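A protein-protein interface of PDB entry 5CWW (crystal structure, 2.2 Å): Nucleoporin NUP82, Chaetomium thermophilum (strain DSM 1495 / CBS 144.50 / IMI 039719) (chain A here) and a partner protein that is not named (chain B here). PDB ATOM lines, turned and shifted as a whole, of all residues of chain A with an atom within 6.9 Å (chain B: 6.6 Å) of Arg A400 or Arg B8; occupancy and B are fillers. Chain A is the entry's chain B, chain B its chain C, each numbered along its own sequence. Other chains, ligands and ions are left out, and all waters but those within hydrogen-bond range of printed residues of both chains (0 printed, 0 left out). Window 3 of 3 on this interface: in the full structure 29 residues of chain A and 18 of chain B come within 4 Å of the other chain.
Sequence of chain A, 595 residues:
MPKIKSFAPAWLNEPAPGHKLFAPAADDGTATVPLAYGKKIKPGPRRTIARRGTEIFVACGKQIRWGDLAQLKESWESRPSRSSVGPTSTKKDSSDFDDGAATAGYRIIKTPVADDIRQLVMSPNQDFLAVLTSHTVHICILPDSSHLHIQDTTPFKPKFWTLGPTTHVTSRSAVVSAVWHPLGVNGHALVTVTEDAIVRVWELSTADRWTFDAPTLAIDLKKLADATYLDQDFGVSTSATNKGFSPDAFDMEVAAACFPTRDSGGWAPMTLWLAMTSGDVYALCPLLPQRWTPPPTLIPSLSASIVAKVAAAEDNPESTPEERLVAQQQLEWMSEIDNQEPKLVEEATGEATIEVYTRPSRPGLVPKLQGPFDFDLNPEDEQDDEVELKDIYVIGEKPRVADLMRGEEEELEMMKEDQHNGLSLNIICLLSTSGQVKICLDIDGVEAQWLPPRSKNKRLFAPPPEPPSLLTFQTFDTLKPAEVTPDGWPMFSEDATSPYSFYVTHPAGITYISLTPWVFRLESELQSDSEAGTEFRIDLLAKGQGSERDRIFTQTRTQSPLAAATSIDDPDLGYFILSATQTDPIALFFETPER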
ATOM      1  N   GLU A 397      17.438 -14.986 -25.796  1.00  0.00           N
ATOM      2  CA  GLU A 397      17.168 -16.185 -25.018  1.00  0.00           C
ATOM      3  C   GLU A 397      17.591 -15.949 -23.578  1.00  0.00           C
ATOM      4  O   GLU A 397      18.559 -15.231 -23.326  1.00  0.00           O
ATOM      5  CB  GLU A 397      17.911 -17.387 -25.596  1.00  0.00           C
ATOM      6  CG  GLU A 397      19.416 -17.163 -25.736  1.00  0.00           C
ATOM      7  CD  GLU A 397      20.196 -18.450 -25.886  1.00  0.00           C
ATOM      8  OE1 GLU A 397      19.927 -19.407 -25.131  1.00  0.00           O
ATOM      9  OE2 GLU A 397      21.087 -18.500 -26.756  1.00  0.00           O
ATOM     10  N   LYS A 398      16.871 -16.550 -22.638  1.00  0.00           N
ATOM     11  CA  LYS A 398      17.222 -16.433 -21.230  1.00  0.00           C
ATOM     12  C   LYS A 398      17.826 -17.746 -20.746  1.00  0.00           C
ATOM     13  O   LYS A 398      17.453 -18.811 -21.236  1.00  0.00           O
ATOM     14  CB  LYS A 398      15.995 -16.061 -20.399  1.00  0.00           C
ATOM     15  CG  LYS A 398      15.323 -14.768 -20.847  1.00  0.00           C
ATOM     16  CD  LYS A 398      14.451 -14.163 -19.752  1.00  0.00           C
ATOM     17  CE  LYS A 398      15.282 -13.507 -18.653  1.00  0.00           C
ATOM     18  NZ  LYS A 398      16.121 -12.384 -19.165  1.00  0.00           N
ATOM     19  N   PRO A 399      18.773 -17.678 -19.792  1.00  0.00           N
ATOM     20  CA  PRO A 399      19.386 -18.905 -19.268  1.00  0.00           C
ATOM     21  C   PRO A 399      18.358 -19.877 -18.694  1.00  0.00           C
ATOM     22  O   PRO A 399      17.366 -19.449 -18.106  1.00  0.00           O
ATOM     23  CB  PRO A 399      20.320 -18.390 -18.167  1.00  0.00           C
ATOM     24  CG  PRO A 399      20.602 -16.981 -18.534  1.00  0.00           C
ATOM     25  CD  PRO A 399      19.354 -16.471 -19.179  1.00  0.00           C
ATOM     26  N   ARG A 400      18.603 -21.172 -18.868  1.00  0.00           N
ATOM     27  CA  ARG A 400      17.687 -22.197 -18.386  1.00  0.00           C
ATOM     28  C   ARG A 400      17.905 -22.464 -16.901  1.00  0.00           C
ATOM     29  O   ARG A 400      19.034 -22.413 -16.410  1.00  0.00           O
ATOM     30  CB  ARG A 400      17.863 -23.490 -19.185  1.00  0.00           C
ATOM     31  CG  ARG A 400      17.819 -23.299 -20.694  1.00  0.00           C
ATOM     32  CD  ARG A 400      18.047 -24.613 -21.423  1.00  0.00           C
ATOM     33  NE  ARG A 400      18.324 -24.415 -22.843  1.00  0.00           N
ATOM     34  CZ  ARG A 400      18.637 -25.391 -23.690  1.00  0.00           C
ATOM     35  NH1 ARG A 400      18.716 -26.646 -23.266  1.00  0.00           N
ATOM     36  NH2 ARG A 400      18.874 -25.113 -24.965  1.00  0.00           N
ATOM     37  N   SER A 424      13.650 -19.797 -23.726  1.00  0.00           N
ATOM     38  CA  SER A 424      15.013 -20.211 -24.044  1.00  0.00           C
ATOM     39  C   SER A 424      15.317 -20.095 -25.540  1.00  0.00           C
ATOM     40  O   SER A 424      16.063 -20.902 -26.093  1.00  0.00           O
ATOM     41  CB  SER A 424      15.248 -21.649 -23.576  1.00  0.00           C
ATOM     42  OG  SER A 424      14.306 -22.535 -24.157  1.00  0.00           O
ATOM     43  N   LEU A 425      14.741 -19.085 -26.187  1.00  0.00           N
ATOM     44  CA  LEU A 425      14.978 -18.831 -27.603  1.00  0.00           C
ATOM     45  C   LEU A 425      15.022 -17.336 -27.855  1.00  0.00           C
ATOM     46  O   LEU A 425      14.290 -16.571 -27.226  1.00  0.00           O
ATOM     47  CB  LEU A 425      13.880 -19.452 -28.469  1.00  0.00           C
ATOM     48  CG  LEU A 425      13.648 -20.963 -28.429  1.00  0.00           C
ATOM     49  CD1 LEU A 425      12.360 -21.277 -29.163  1.00  0.00           C
ATOM     50  CD2 LEU A 425      14.811 -21.720 -29.047  1.00  0.00           C
ATOM     51  N   ASP A 442      14.132 -17.903 -33.216  1.00  0.00           N
ATOM     52  CA  ASP A 442      15.420 -18.465 -33.595  1.00  0.00           C
ATOM     53  C   ASP A 442      15.495 -19.927 -33.167  1.00  0.00           C
ATOM     54  O   ASP A 442      16.047 -20.256 -32.117  1.00  0.00           O
ATOM     55  CB  ASP A 442      16.559 -17.656 -32.975  1.00  0.00           C
ATOM     56  CG  ASP A 442      17.927 -18.178 -33.366  1.00  0.00           C
ATOM     57  OD1 ASP A 442      18.016 -18.938 -34.356  1.00  0.00           O
ATOM     58  OD2 ASP A 442      18.915 -17.817 -32.691  1.00  0.00           O
ATOM     59  N   ILE A 443      14.924 -20.796 -33.996  1.00  0.00           N
ATOM     60  CA  ILE A 443      14.855 -22.225 -33.714  1.00  0.00           C
ATOM     61  C   ILE A 443      16.229 -22.882 -33.761  1.00  0.00           C
ATOM     62  O   ILE A 443      16.532 -23.768 -32.963  1.00  0.00           O
ATOM     63  CB  ILE A 443      13.932 -22.943 -34.725  1.00  0.00           C
ATOM     64  CG1 ILE A 443      12.543 -22.296 -34.744  1.00  0.00           C
ATOM     65  CG2 ILE A 443      13.827 -24.430 -34.410  1.00  0.00           C
ATOM     66  CD1 ILE A 443      11.839 -22.279 -33.401  1.00  0.00           C
ATOM     67  N   GLU A 523       7.888 -22.298 -23.470  1.00  0.00           N
ATOM     68  CA  GLU A 523       9.034 -22.684 -22.652  1.00  0.00           C
ATOM     69  C   GLU A 523       8.697 -23.866 -21.744  1.00  0.00           C
ATOM     70  O   GLU A 523       9.525 -24.755 -21.542  1.00  0.00           O
ATOM     71  CB  GLU A 523       9.520 -21.501 -21.811  1.00  0.00           C
ATOM     72  CG  GLU A 523      10.689 -21.833 -20.882  1.00  0.00           C
ATOM     73  CD  GLU A 523      11.939 -22.263 -21.630  1.00  0.00           C
ATOM     74  OE1 GLU A 523      12.036 -21.987 -22.844  1.00  0.00           O
ATOM     75  OE2 GLU A 523      12.824 -22.887 -21.006  1.00  0.00           O
ATOM     76  N   LEU A 526       8.894 -26.888 -23.712  1.00  0.00           N
ATOM     77  CA  LEU A 526      10.291 -27.217 -23.974  1.00  0.00           C
ATOM     78  C   LEU A 526      10.923 -27.889 -22.760  1.00  0.00           C
ATOM     79  O   LEU A 526      11.805 -28.735 -22.899  1.00  0.00           O
ATOM     80  CB  LEU A 526      11.087 -25.963 -24.352  1.00  0.00           C
ATOM     81  CG  LEU A 526      10.769 -25.352 -25.720  1.00  0.00           C
ATOM     82  CD1 LEU A 526      11.421 -23.984 -25.860  1.00  0.00           C
ATOM     83  CD2 LEU A 526      11.214 -26.275 -26.849  1.00  0.00           C
ATOM     84  N   GLN A 527      10.459 -27.512 -21.573  1.00  0.00           N
ATOM     85  CA  GLN A 527      10.953 -28.099 -20.332  1.00  0.00           C
ATOM     86  C   GLN A 527      10.047 -29.225 -19.839  1.00  0.00           C
ATOM     87  O   GLN A 527      10.210 -29.708 -18.720  1.00  0.00           O
ATOM     88  CB  GLN A 527      11.074 -27.020 -19.254  1.00  0.00           C
ATOM     89  CG  GLN A 527      12.121 -25.962 -19.558  1.00  0.00           C
ATOM     90  CD  GLN A 527      12.262 -24.941 -18.444  1.00  0.00           C
ATOM     91  OE1 GLN A 527      11.586 -25.026 -17.419  1.00  0.00           O
ATOM     92  NE2 GLN A 527      13.136 -23.960 -18.646  1.00  0.00           N
ATOM     93  N   ALA B   3      19.332 -36.406 -23.575  1.00  0.00           N
ATOM     94  CA  ALA B   3      18.329 -36.630 -24.610  1.00  0.00           C
ATOM     95  C   ALA B   3      17.351 -35.460 -24.686  1.00  0.00           C
ATOM     96  O   ALA B   3      16.437 -35.460 -25.511  1.00  0.00           O
ATOM     97  CB  ALA B   3      17.580 -37.928 -24.346  1.00  0.00           C
ATOM     98  N   ARG B   4      17.544 -34.467 -23.825  1.00  0.00           N
ATOM     99  CA  ARG B   4      16.665 -33.305 -23.796  1.00  0.00           C
ATOM    100  C   ARG B   4      16.824 -32.463 -25.057  1.00  0.00           C
ATOM    101  O   ARG B   4      15.896 -31.765 -25.465  1.00  0.00           O
ATOM    102  CB  ARG B   4      16.948 -32.453 -22.558  1.00  0.00           C
ATOM    103  CG  ARG B   4      16.696 -33.181 -21.246  1.00  0.00           C
ATOM    104  CD  ARG B   4      16.398 -32.212 -20.115  1.00  0.00           C
ATOM    105  NE  ARG B   4      16.335 -32.884 -18.819  1.00  0.00           N
ATOM    106  CZ  ARG B   4      17.350 -32.987 -17.963  1.00  0.00           C
ATOM    107  NH1 ARG B   4      18.536 -32.465 -18.247  1.00  0.00           N
ATOM    108  NH2 ARG B   4      17.177 -33.620 -16.811  1.00  0.00           N
ATOM    109  N   GLU B   5      18.000 -32.531 -25.673  1.00  0.00           N
ATOM    110  CA  GLU B   5      18.258 -31.772 -26.890  1.00  0.00           C
ATOM    111  C   GLU B   5      17.419 -32.315 -28.040  1.00  0.00           C
ATOM    112  O   GLU B   5      16.850 -31.551 -28.820  1.00  0.00           O
ATOM    113  CB  GLU B   5      19.743 -31.814 -27.252  1.00  0.00           C
ATOM    114  CG  GLU B   5      20.126 -30.874 -28.387  1.00  0.00           C
ATOM    115  CD  GLU B   5      19.846 -29.418 -28.061  1.00  0.00           C
ATOM    116  OE1 GLU B   5      19.938 -29.046 -26.872  1.00  0.00           O
ATOM    117  OE2 GLU B   5      19.529 -28.650 -28.992  1.00  0.00           O
ATOM    118  N   ALA B   6      17.346 -33.639 -28.137  1.00  0.00           N
ATOM    119  CA  ALA B   6      16.517 -34.289 -29.144  1.00  0.00           C
ATOM    120  C   ALA B   6      15.046 -33.962 -28.910  1.00  0.00           C
ATOM    121  O   ALA B   6      14.262 -33.870 -29.855  1.00  0.00           O
ATOM    122  CB  ALA B   6      16.736 -35.793 -29.126  1.00  0.00           C
ATOM    123  N   LYS B   7      14.683 -33.786 -27.643  1.00  0.00           N
ATOM    124  CA  LYS B   7      13.317 -33.436 -27.277  1.00  0.00           C
ATOM    125  C   LYS B   7      13.021 -31.991 -27.670  1.00  0.00           C
ATOM    126  O   LYS B   7      11.943 -31.689 -28.184  1.00  0.00           O
ATOM    127  CB  LYS B   7      13.092 -33.645 -25.777  1.00  0.00           C
ATOM    128  CG  LYS B   7      11.633 -33.605 -25.355  1.00  0.00           C
ATOM    129  CD  LYS B   7      11.469 -34.022 -23.902  1.00  0.00           C
ATOM    130  CE  LYS B   7      10.013 -34.293 -23.552  1.00  0.00           C
ATOM    131  NZ  LYS B   7       9.866 -34.864 -22.182  1.00  0.00           N
ATOM    132  N   ARG B   8      13.978 -31.101 -27.423  1.00  0.00           N
ATOM    133  CA  ARG B   8      13.853 -29.710 -27.848  1.00  0.00           C
ATOM    134  C   ARG B   8      13.726 -29.627 -29.363  1.00  0.00           C
ATOM    135  O   ARG B   8      12.832 -28.962 -29.886  1.00  0.00           O
ATOM    136  CB  ARG B   8      15.058 -28.885 -27.388  1.00  0.00           C
ATOM    137  CG  ARG B   8      15.032 -28.489 -25.921  1.00  0.00           C
ATOM    138  CD  ARG B   8      16.275 -27.692 -25.545  1.00  0.00           C
ATOM    139  NE  ARG B   8      16.406 -26.463 -26.326  1.00  0.00           N
ATOM    140  CZ  ARG B   8      15.849 -25.298 -26.003  1.00  0.00           C
ATOM    141  NH1 ARG B   8      15.113 -25.187 -24.907  1.00  0.00           N
ATOM    142  NH2 ARG B   8      16.027 -24.239 -26.781  1.00  0.00           N
ATOM    143  N   LYS B   9      14.631 -30.310 -30.056  1.00  0.00           N
ATOM    144  CA  LYS B   9      14.670 -30.294 -31.512  1.00  0.00           C
ATOM    145  C   LYS B   9      13.355 -30.795 -32.104  1.00  0.00           C
ATOM    146  O   LYS B   9      12.827 -30.208 -33.048  1.00  0.00           O
ATOM    147  CB  LYS B   9      15.835 -31.145 -32.020  1.00  0.00           C
ATOM    148  CG  LYS B   9      16.131 -30.975 -33.503  1.00  0.00           C
ATOM    149  CD  LYS B   9      17.397 -31.719 -33.908  1.00  0.00           C
ATOM    150  CE  LYS B   9      17.815 -31.374 -35.331  1.00  0.00           C
ATOM    151  NZ  LYS B   9      19.033 -32.118 -35.761  1.00  0.00           N
ATOM    152  N   ALA B  10      12.831 -31.878 -31.540  1.00  0.00           N
ATOM    153  CA  ALA B  10      11.574 -32.454 -32.005  1.00  0.00           C
ATOM    154  C   ALA B  10      10.398 -31.523 -31.722  1.00  0.00           C
ATOM    155  O   ALA B  10       9.529 -31.331 -32.573  1.00  0.00           O
ATOM    156  CB  ALA B  10      11.343 -33.808 -31.352  1.00  0.00           C
ATOM    157  N   THR B  11      10.377 -30.955 -30.520  1.00  0.00           N
ATOM    158  CA  THR B  11       9.314 -30.040 -30.110  1.00  0.00           C
ATOM    159  C   THR B  11       9.210 -28.840 -31.046  1.00  0.00           C
ATOM    160  O   THR B  11       8.116 -28.454 -31.460  1.00  0.00           O
ATOM    161  CB  THR B  11       9.541 -29.526 -28.675  1.00  0.00           C
ATOM    162  OG1 THR B  11       9.697 -30.637 -27.785  1.00  0.00           O
ATOM    163  CG2 THR B  11       8.371 -28.666 -28.211  1.00  0.00           C
ATOM    164  N   LEU B  12      10.354 -28.246 -31.368  1.00  0.00           N
ATOM    165  CA  LEU B  12      10.384 -27.066 -32.221  1.00  0.00           C
ATOM    166  C   LEU B  12      10.069 -27.441 -33.667  1.00  0.00           C
ATOM    167  O   LEU B  12       9.441 -26.668 -34.392  1.00  0.00           O
ATOM    168  CB  LEU B  12      11.743 -26.371 -32.120  1.00  0.00           C
ATOM    169  CG  LEU B  12      12.059 -25.807 -30.728  1.00  0.00           C
ATOM    170  CD1 LEU B  12      13.505 -25.355 -30.622  1.00  0.00           C
ATOM    171  CD2 LEU B  12      11.123 -24.657 -30.381  1.00  0.00           C
ATOM    172  N   ARG B  13      10.507 -28.626 -34.082  1.00  0.00           N
ATOM    173  CA  ARG B  13      10.121 -29.161 -35.382  1.00  0.00           C
ATOM    174  C   ARG B  13       8.600 -29.263 -35.474  1.00  0.00           C
ATOM    175  O   ARG B  13       8.011 -28.982 -36.517  1.00  0.00           O
ATOM    176  CB  ARG B  13      10.753 -30.534 -35.622  1.00  0.00           C
ATOM    177  CG  ARG B  13      12.119 -30.499 -36.291  1.00  0.00           C
ATOM    178  CD  ARG B  13      12.377 -31.792 -37.052  1.00  0.00           C
ATOM    179  NE  ARG B  13      13.637 -31.766 -37.793  1.00  0.00           N
ATOM    180  CZ  ARG B  13      14.778 -32.320 -37.386  1.00  0.00           C
ATOM    181  NH1 ARG B  13      14.849 -32.961 -36.226  1.00  0.00           N
ATOM    182  NH2 ARG B  13      15.859 -32.232 -38.149  1.00  0.00           N
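The guanidinium group (NH2) of Arg A400 lies close to the guanidinium group (NE) of Arg B8. The side-chain hydroxyl (OG) of Ser A424 sits at hydrogen-bond distance from the guanidinium group (NH1) of Arg B8, 2.9 Å away.
OG of Ser A424 lies within hydrogen-bond range of OE1 of Glu A523, at 2.7 Å. O of Lys B7 lies within hydrogen-bond range of OG1 of Thr B11 (2.5 Å).
Among the printed residues, pairs that only touch across the chains: Leu A425 with Arg B8 (3.6 Å), Ile A443 with Leu B12 (3.7 Å), Leu A425 with Leu B12 (3.8 Å), Leu A526 with Leu B12 (3.9 Å), Leu A526 with Thr B11 (3.96 Å) and Leu A526 with Arg B8 (3.998 Å).
Of chain B, only Arg B8 comes within 4 Å of Arg A400. Of the printed residues of chain B, Leu A425 touches Arg B8 and Leu B12. Printed residues of chain B within 4 Å of Ile A443: Leu B12 (3.7 Å). Glu A523 touches none of the printed residues of chain B. Printed residues of chain B within 4 Å of Leu A526: Arg B8 (3.998 Å), Thr B11 (3.96 Å) and Leu B12 (3.9 Å). Glu B5 touches none of the printed residues of chain A. Printed residues of chain A within 4 Å of Leu B12: Leu A425 (3.8 Å), Ile A443 (3.7 Å) and Leu A526 (3.9 Å). The nearest residue of chain B that does not touch Arg A400 is Glu B5 (4.5 Å). The nearest printed residue of chain A that does not touch Arg B8 is Glu A523 (4.9 Å). The nearest printed residue of chain A that does not touch Leu B12 is Asp A442 (5.9 Å).
Hydrophobic or aromatic side chains of chain A within 4 Å of the printed part of chain B: Leu A425, Ile A443 and Leu A526. Along chain A the printed residues that touch a printed residue of chain B span positions 400 to 526. Among the printed residues, 8 pairs touch across the chains.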
